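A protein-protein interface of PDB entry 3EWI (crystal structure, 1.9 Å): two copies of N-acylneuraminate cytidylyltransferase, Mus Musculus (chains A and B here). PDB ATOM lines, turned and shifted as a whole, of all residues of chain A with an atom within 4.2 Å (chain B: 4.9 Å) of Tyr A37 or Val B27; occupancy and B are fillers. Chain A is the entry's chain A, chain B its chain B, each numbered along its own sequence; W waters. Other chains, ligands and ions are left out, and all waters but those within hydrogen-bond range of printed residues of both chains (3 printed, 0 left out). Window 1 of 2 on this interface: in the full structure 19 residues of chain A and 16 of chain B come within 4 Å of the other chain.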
ATOM      1  N   LEU A  20      -5.831  32.578 -11.256  1.00  0.00           N
ATOM      2  CA  LEU A  20      -4.572  32.146 -10.700  1.00  0.00           C
ATOM      3  C   LEU A  20      -4.789  31.138  -9.556  1.00  0.00           C
ATOM      4  O   LEU A  20      -4.177  30.081  -9.539  1.00  0.00           O
ATOM      5  CB  LEU A  20      -3.684  33.308 -10.268  1.00  0.00           C
ATOM      6  CG  LEU A  20      -2.407  32.942  -9.494  1.00  0.00           C
ATOM      7  CD1 LEU A  20      -1.319  32.430 -10.438  1.00  0.00           C
ATOM      8  CD2 LEU A  20      -1.919  34.145  -8.721  1.00  0.00           C
ATOM      9  N   GLU A  33      -4.889  31.351   6.508  1.00  0.00           N
ATOM     10  CA  GLU A  33      -5.694  30.752   5.456  1.00  0.00           C
ATOM     11  C   GLU A  33      -4.835  30.197   4.360  1.00  0.00           C
ATOM     12  O   GLU A  33      -3.764  30.737   4.062  1.00  0.00           O
ATOM     13  CB  GLU A  33      -6.659  31.764   4.845  1.00  0.00           C
ATOM     14  CG  GLU A  33      -7.819  32.136   5.745  1.00  0.00           C
ATOM     15  CD  GLU A  33      -8.565  33.334   5.216  1.00  0.00           C
ATOM     16  OE1 GLU A  33      -8.105  33.911   4.214  1.00  0.00           O
ATOM     17  OE2 GLU A  33      -9.602  33.690   5.801  1.00  0.00           O
ATOM     18  N   ILE A  34      -5.337  29.116   3.762  1.00  0.00           N
ATOM     19  CA  ILE A  34      -4.672  28.421   2.684  1.00  0.00           C
ATOM     20  C   ILE A  34      -5.376  28.673   1.352  1.00  0.00           C
ATOM     21  O   ILE A  34      -6.601  28.708   1.278  1.00  0.00           O
ATOM     22  CB  ILE A  34      -4.580  26.897   3.000  1.00  0.00           C
ATOM     23  CG1 ILE A  34      -3.686  26.681   4.233  1.00  0.00           C
ATOM     24  CG2 ILE A  34      -4.065  26.127   1.805  1.00  0.00           C
ATOM     25  CD1 ILE A  34      -3.278  25.251   4.503  1.00  0.00           C
ATOM     26  N   ILE A  35      -4.583  28.854   0.304  1.00  0.00           N
ATOM     27  CA  ILE A  35      -5.099  28.976  -1.047  1.00  0.00           C
ATOM     28  C   ILE A  35      -4.404  27.936  -1.904  1.00  0.00           C
ATOM     29  O   ILE A  35      -3.384  27.371  -1.495  1.00  0.00           O
ATOM     30  CB  ILE A  35      -4.865  30.417  -1.631  1.00  0.00           C
ATOM     31  CG1 ILE A  35      -3.367  30.772  -1.664  1.00  0.00           C
ATOM     32  CG2 ILE A  35      -5.686  31.434  -0.880  1.00  0.00           C
ATOM     33  CD1 ILE A  35      -2.997  31.794  -2.721  1.00  0.00           C
ATOM     34  N   SER A  36      -4.944  27.676  -3.078  1.00  0.00           N
ATOM     35  CA  SER A  36      -4.427  26.627  -3.934  1.00  0.00           C
ATOM     36  C   SER A  36      -4.221  27.111  -5.348  1.00  0.00           C
ATOM     37  O   SER A  36      -5.063  27.815  -5.902  1.00  0.00           O
ATOM     38  CB  SER A  36      -5.388  25.412  -3.936  1.00  0.00           C
ATOM     39  OG  SER A  36      -4.810  24.306  -4.619  1.00  0.00           O
ATOM     40  N   TYR A  37      -3.117  26.680  -5.947  1.00  0.00           N
ATOM     41  CA  TYR A  37      -2.827  26.963  -7.346  1.00  0.00           C
ATOM     42  C   TYR A  37      -2.150  25.727  -7.970  1.00  0.00           C
ATOM     43  O   TYR A  37      -1.921  24.754  -7.270  1.00  0.00           O
ATOM     44  CB  TYR A  37      -1.918  28.195  -7.440  1.00  0.00           C
ATOM     45  CG  TYR A  37      -0.495  27.977  -6.976  1.00  0.00           C
ATOM     46  CD1 TYR A  37      -0.171  28.005  -5.628  1.00  0.00           C
ATOM     47  CD2 TYR A  37       0.530  27.778  -7.896  1.00  0.00           C
ATOM     48  CE1 TYR A  37       1.114  27.831  -5.196  1.00  0.00           C
ATOM     49  CE2 TYR A  37       1.819  27.594  -7.480  1.00  0.00           C
ATOM     50  CZ  TYR A  37       2.111  27.626  -6.126  1.00  0.00           C
ATOM     51  OH  TYR A  37       3.388  27.449  -5.716  1.00  0.00           O
ATOM     52  N   ASP A  38      -1.863  25.784  -9.272  1.00  0.00           N
ATOM     53  CA  ASP A  38      -1.296  24.671 -10.048  1.00  0.00           C
ATOM     54  C   ASP A  38       0.078  25.085 -10.552  1.00  0.00           C
ATOM     55  O   ASP A  38       0.244  26.168 -11.127  1.00  0.00           O
ATOM     56  CB  ASP A  38      -2.210  24.356 -11.244  1.00  0.00           C
ATOM     57  CG  ASP A  38      -1.966  22.985 -11.848  1.00  0.00           C
ATOM     58  OD1 ASP A  38      -0.793  22.566 -12.001  1.00  0.00           O
ATOM     59  OD2 ASP A  38      -2.972  22.352 -12.217  1.00  0.00           O
ATOM     60  N   ALA A  42       2.008  28.387 -12.771  1.00  0.00           N
ATOM     61  CA  ALA A  42       3.234  29.095 -12.392  1.00  0.00           C
ATOM     62  C   ALA A  42       4.319  28.972 -13.464  1.00  0.00           C
ATOM     63  O   ALA A  42       4.993  29.947 -13.804  1.00  0.00           O
ATOM     64  CB  ALA A  42       3.746  28.603 -11.021  1.00  0.00           C
ATOM     65  N   ALA A  70       4.455  33.856  -1.827  1.00  0.00           N
ATOM     66  CA  ALA A  70       4.719  32.423  -1.641  1.00  0.00           C
ATOM     67  C   ALA A  70       4.627  31.635  -2.959  1.00  0.00           C
ATOM     68  O   ALA A  70       5.147  30.523  -3.051  1.00  0.00           O
ATOM     69  CB  ALA A  70       3.777  31.848  -0.617  1.00  0.00           C
ATOM     70  N   LEU A  71       3.978  32.213  -3.971  1.00  0.00           N
ATOM     71  CA  LEU A  71       3.903  31.583  -5.295  1.00  0.00           C
ATOM     72  C   LEU A  71       5.167  31.773  -6.133  1.00  0.00           C
ATOM     73  O   LEU A  71       5.362  31.055  -7.120  1.00  0.00           O
ATOM     74  CB  LEU A  71       2.681  32.066  -6.059  1.00  0.00           C
ATOM     75  CG  LEU A  71       1.354  31.336  -5.807  1.00  0.00           C
ATOM     76  CD1 LEU A  71       0.849  31.512  -4.365  1.00  0.00           C
ATOM     77  CD2 LEU A  71       0.266  31.750  -6.825  1.00  0.00           C
ATOM     78  N   GLY A 144      -7.110  28.067 -11.389  1.00  0.00           N
ATOM     79  CA  GLY A 144      -6.134  27.546 -10.455  1.00  0.00           C
ATOM     80  C   GLY A 144      -5.729  26.111 -10.785  1.00  0.00           C
ATOM     81  O   GLY A 144      -5.020  25.481 -10.015  1.00  0.00           O
ATOM     82  N   ARG A 145      -6.200  25.601 -11.918  1.00  0.00           N
ATOM     83  CA  ARG A 145      -5.972  24.198 -12.300  1.00  0.00           C
ATOM     84  C   ARG A 145      -5.632  24.061 -13.790  1.00  0.00           C
ATOM     85  O   ARG A 145      -6.088  23.137 -14.481  1.00  0.00           O
ATOM     86  CB  ARG A 145      -7.197  23.355 -11.936  1.00  0.00           C
ATOM     87  CG  ARG A 145      -7.457  23.252 -10.446  1.00  0.00           C
ATOM     88  CD  ARG A 145      -6.312  22.535  -9.737  1.00  0.00           C
ATOM     89  NE  ARG A 145      -6.556  22.214  -8.326  1.00  0.00           N
ATOM     90  CZ  ARG A 145      -6.068  22.884  -7.288  1.00  0.00           C
ATOM     91  NH1 ARG A 145      -5.308  23.948  -7.476  1.00  0.00           N
ATOM     92  NH2 ARG A 145      -6.322  22.473  -6.041  1.00  0.00           N
ATOM     93  N   GLY B  23       0.473  18.145  -9.006  1.00  0.00           N
ATOM     94  CA  GLY B  23       0.912  19.510  -9.345  1.00  0.00           C
ATOM     95  C   GLY B  23       0.168  20.600  -8.586  1.00  0.00           C
ATOM     96  O   GLY B  23       0.551  21.759  -8.662  1.00  0.00           O
ATOM     97  N   HIS B  24      -0.889  20.234  -7.855  1.00  0.00           N
ATOM     98  CA  HIS B  24      -1.562  21.156  -6.931  1.00  0.00           C
ATOM     99  C   HIS B  24      -0.687  21.521  -5.739  1.00  0.00           C
ATOM    100  O   HIS B  24      -0.039  20.667  -5.129  1.00  0.00           O
ATOM    101  CB  HIS B  24      -2.916  20.595  -6.449  1.00  0.00           C
ATOM    102  CG  HIS B  24      -3.786  20.062  -7.547  1.00  0.00           C
ATOM    103  ND1 HIS B  24      -4.885  19.263  -7.302  1.00  0.00           N
ATOM    104  CD2 HIS B  24      -3.705  20.190  -8.890  1.00  0.00           C
ATOM    105  CE1 HIS B  24      -5.448  18.933  -8.450  1.00  0.00           C
ATOM    106  NE2 HIS B  24      -4.754  19.488  -9.429  1.00  0.00           N
ATOM    107  N   ILE B  25      -0.633  22.818  -5.431  1.00  0.00           N
ATOM    108  CA  ILE B  25       0.033  23.282  -4.215  1.00  0.00           C
ATOM    109  C   ILE B  25      -1.009  23.983  -3.379  1.00  0.00           C
ATOM    110  O   ILE B  25      -1.872  24.687  -3.915  1.00  0.00           O
ATOM    111  CB  ILE B  25       1.204  24.223  -4.536  1.00  0.00           C
ATOM    112  CG1 ILE B  25       2.291  23.448  -5.291  1.00  0.00           C
ATOM    113  CG2 ILE B  25       1.804  24.848  -3.238  1.00  0.00           C
ATOM    114  CD1 ILE B  25       3.046  24.306  -6.247  1.00  0.00           C
ATOM    115  N   TYR B  26      -0.940  23.761  -2.072  1.00  0.00           N
ATOM    116  CA  TYR B  26      -1.761  24.458  -1.100  1.00  0.00           C
ATOM    117  C   TYR B  26      -0.768  25.226  -0.262  1.00  0.00           C
ATOM    118  O   TYR B  26       0.174  24.651   0.288  1.00  0.00           O
ATOM    119  CB  TYR B  26      -2.542  23.448  -0.238  1.00  0.00           C
ATOM    120  CG  TYR B  26      -3.506  22.622  -1.068  1.00  0.00           C
ATOM    121  CD1 TYR B  26      -4.824  23.030  -1.223  1.00  0.00           C
ATOM    122  CD2 TYR B  26      -3.076  21.467  -1.728  1.00  0.00           C
ATOM    123  CE1 TYR B  26      -5.710  22.321  -2.015  1.00  0.00           C
ATOM    124  CE2 TYR B  26      -3.955  20.721  -2.514  1.00  0.00           C
ATOM    125  CZ  TYR B  26      -5.285  21.167  -2.646  1.00  0.00           C
ATOM    126  OH  TYR B  26      -6.185  20.477  -3.419  1.00  0.00           O
ATOM    127  N   VAL B  27      -0.930  26.535  -0.220  1.00  0.00           N
ATOM    128  CA  VAL B  27       0.064  27.377   0.446  1.00  0.00           C
ATOM    129  C   VAL B  27      -0.568  28.413   1.360  1.00  0.00           C
ATOM    130  O   VAL B  27      -1.643  28.970   1.073  1.00  0.00           O
ATOM    131  CB  VAL B  27       1.030  28.020  -0.597  1.00  0.00           C
ATOM    132  CG1 VAL B  27       0.289  29.021  -1.485  1.00  0.00           C
ATOM    133  CG2 VAL B  27       2.266  28.619   0.074  1.00  0.00           C
ATOM    134  N   SER B  28       0.130  28.682   2.462  1.00  0.00           N
ATOM    135  CA  SER B  28      -0.273  29.682   3.430  1.00  0.00           C
ATOM    136  C   SER B  28       0.631  30.933   3.370  1.00  0.00           C
ATOM    137  O   SER B  28       1.723  30.915   2.777  1.00  0.00           O
ATOM    138  CB  SER B  28      -0.223  29.048   4.830  1.00  0.00           C
ATOM    139  OG  SER B  28      -1.380  29.376   5.576  1.00  0.00           O
ATOM    140  N   GLY B  29       0.166  32.011   3.984  1.00  0.00           N
ATOM    141  CA  GLY B  29       0.928  33.267   4.082  1.00  0.00           C
ATOM    142  C   GLY B  29       2.261  33.131   4.805  1.00  0.00           C
ATOM    143  O   GLY B  29       3.183  33.905   4.551  1.00  0.00           O
ATOM    144  N   GLN B  31       4.077  30.681   4.294  1.00  0.00           N
ATOM    145  CA  GLN B  31       4.753  29.837   3.292  1.00  0.00           C
ATOM    146  C   GLN B  31       4.779  28.321   3.590  1.00  0.00           C
ATOM    147  O   GLN B  31       5.533  27.560   2.968  1.00  0.00           O
ATOM    148  CB  GLN B  31       6.130  30.408   2.905  1.00  0.00           C
ATOM    149  CG  GLN B  31       6.017  31.805   2.274  1.00  0.00           C
ATOM    150  CD  GLN B  31       7.296  32.297   1.618  1.00  0.00           C
ATOM    151  OE1 GLN B  31       8.286  31.567   1.525  1.00  0.00           O
ATOM    152  NE2 GLN B  31       7.277  33.552   1.152  1.00  0.00           N
ATOM    153  N   LYS B  32       3.933  27.881   4.518  1.00  0.00           N
ATOM    154  CA  LYS B  32       3.734  26.449   4.727  1.00  0.00           C
ATOM    155  C   LYS B  32       2.978  25.871   3.528  1.00  0.00           C
ATOM    156  O   LYS B  32       2.017  26.479   3.056  1.00  0.00           O
ATOM    157  CB  LYS B  32       3.005  26.183   6.050  1.00  0.00           C
ATOM    158  CG  LYS B  32       1.499  26.004   5.962  1.00  0.00           C
ATOM    159  N   GLU B  33       3.436  24.727   3.021  1.00  0.00           N
ATOM    160  CA  GLU B  33       2.810  24.106   1.851  1.00  0.00           C
ATOM    161  C   GLU B  33       2.350  22.714   2.178  1.00  0.00           C
ATOM    162  O   GLU B  33       3.028  21.976   2.910  1.00  0.00           O
ATOM    163  CB  GLU B  33       3.759  24.022   0.656  1.00  0.00           C
ATOM    164  CG  GLU B  33       4.131  25.358   0.016  1.00  0.00           C
ATOM    165  CD  GLU B  33       5.138  25.205  -1.119  1.00  0.00           C
ATOM    166  OE1 GLU B  33       5.669  24.079  -1.300  1.00  0.00           O
ATOM    167  OE2 GLU B  33       5.406  26.215  -1.820  1.00  0.00           O
ATOM    168  N   ARG B  61      11.540  23.549  -8.813  1.00  0.00           N
ATOM    169  CA  ARG B  61      10.935  24.425  -7.805  1.00  0.00           C
ATOM    170  C   ARG B  61      11.662  24.440  -6.463  1.00  0.00           C
ATOM    171  O   ARG B  61      12.371  23.506  -6.095  1.00  0.00           O
ATOM    172  CB  ARG B  61       9.440  24.071  -7.612  1.00  0.00           C
ATOM    173  CG  ARG B  61       8.670  25.023  -6.685  1.00  0.00           C
ATOM    174  CD  ARG B  61       7.150  24.852  -6.738  1.00  0.00           C
ATOM    175  NE  ARG B  61       6.713  23.590  -6.124  1.00  0.00           N
ATOM    176  CZ  ARG B  61       6.476  23.410  -4.827  1.00  0.00           C
ATOM    177  NH1 ARG B  61       6.621  24.411  -3.966  1.00  0.00           N
ATOM    178  NH2 ARG B  61       6.078  22.227  -4.396  1.00  0.00           N
HETATM  179  O   HOH W   1       4.207  28.060  -3.414  1.00  0.00           O
HETATM  180  O   HOH W   2      -2.296  32.639   5.064  1.00  0.00           O
HETATM  181  O   HOH W   3      -8.500  20.187  -5.677  1.00  0.00           O
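The backbone carbonyl oxygen (O) of Glu A33 is in hydrogen-bond range of the side-chain hydroxyl (OG) of Ser B28 (3.1 Å).
The backbone NH of Val B27 is in hydrogen-bond range of the backbone carbonyl oxygen of Ile A35, at 2.9 Å.
OG of Ser A36 lies within hydrogen-bond range of O of Ile B25 (3.0 Å).
The backbone carbonyl oxygen (O) of Tyr A37 is in hydrogen-bond range of the backbone NH (N) of Ile B25 (3.0 Å).
A ring nitrogen (NE2) of His B24 sits close to the guanidinium group (NE) of Arg A145, at 3.4 Å.
The side-chain hydroxyl of Tyr B26 is in hydrogen-bond range of the guanidinium group of Arg A145, 3.3 Å away.
The side-chain hydroxyl (OG) of Ser A36 is in hydrogen-bond range of the guanidinium group (NH2) of Arg A145, at 2.8 Å.
The backbone carbonyl oxygen (O) of Tyr A37 lies within hydrogen-bond range of the guanidinium group (NH1) of Arg A145, at 3.5 Å.
N of Asp A38 lies within hydrogen-bond range of O of Gly A144 (3.3 Å).
Among the printed residues, pairs that only touch across the chains: Ile A34 with Tyr B26 (3.7 Å), Ile A34 with Val B27 (3.5 Å), Ile A34 with Ser B28 (3.8 Å), Ile A35 with Ile B25 (3.9 Å), Ile A35 with Tyr B26 (3.4 Å), Ser A36 with Tyr B26 (3.4 Å), Tyr A37 with His B24 (3.6 Å), Tyr A37 with Val B27 (3.98 Å), Asp A38 with Gly B23 (3.7 Å), Ala A70 with Val B27 (3.6 Å), Ala A70 with Gln B31 (3.7 Å) and Leu A71 with Val B27 (3.8 Å).
Of the printed residues of chain B, Tyr A37 touches His B24 (3.6 Å), Ile B25 (3.0 Å) and Val B27 (3.98 Å).
Printed residues of chain A within 4 Å of Val B27: Ile A34 (3.5 Å), Ile A35 (2.9 Å), Tyr A37 (3.98 Å), Ala A70 (3.6 Å) and Leu A71 (3.8 Å).
Printed residues of chain A within 4 Å of Ser B28: Glu A33 and Ile A34.
Printed residues of chain A within 4 Å of Ile B25: Ile A35, Ser A36 and Tyr A37.
Of the printed residues of chain A, Gly B23 touches Asp A38.
Printed residues of chain B within 4 Å of Ile A35: Ile B25, Tyr B26 and Val B27.
Printed residues of chain B within 4 Å of Arg A145: His B24 (3.4 Å) and Tyr B26 (3.3 Å).
Gly B29 touches none of the printed residues of chain A.
The nearest printed residue of chain B that does not touch Tyr A37 is Gly B23 (4.1 Å).
The nearest printed residue of chain A that does not touch Val B27 is Glu A33 (4.1 Å).
Of the 11 printed residues of chain B, 7 touch a printed residue of chain A.
Hydrophobic or aromatic side chains of chain B that line the printed part of chain A: His B24, Ile B25, Tyr B26 and Val B27.
Printed residues of chain A that touch a printed residue of chain B: Glu A33, Ile A34, Ile A35, Ser A36, Tyr A37, Asp A38, Ala A70, Leu A71 and Arg A145.
Position printed for both chains: 33.
Of the 18 pairs that touch across the chains among the printed residues, none has its exchanged pair printed and touching as well.
Water W1 lies within hydrogen-bond range of the side-chain hydroxyl (OH) of Tyr A37, the backbone carbonyl oxygen (O) of Ala A70 and the side-chain carboxylate (OE2) of Glu B33.
Water W2 lies within hydrogen-bond range of the backbone carbonyl oxygen of Glu A33 (2.6 Å), the backbone NH of Gly B29 (2.8 Å) and the side-chain hydroxyl of Ser B28 (3.4 Å).
Water W3 bridges NH2 of Arg A145 (3.2 Å) and OH of Tyr B26 (3.2 Å).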
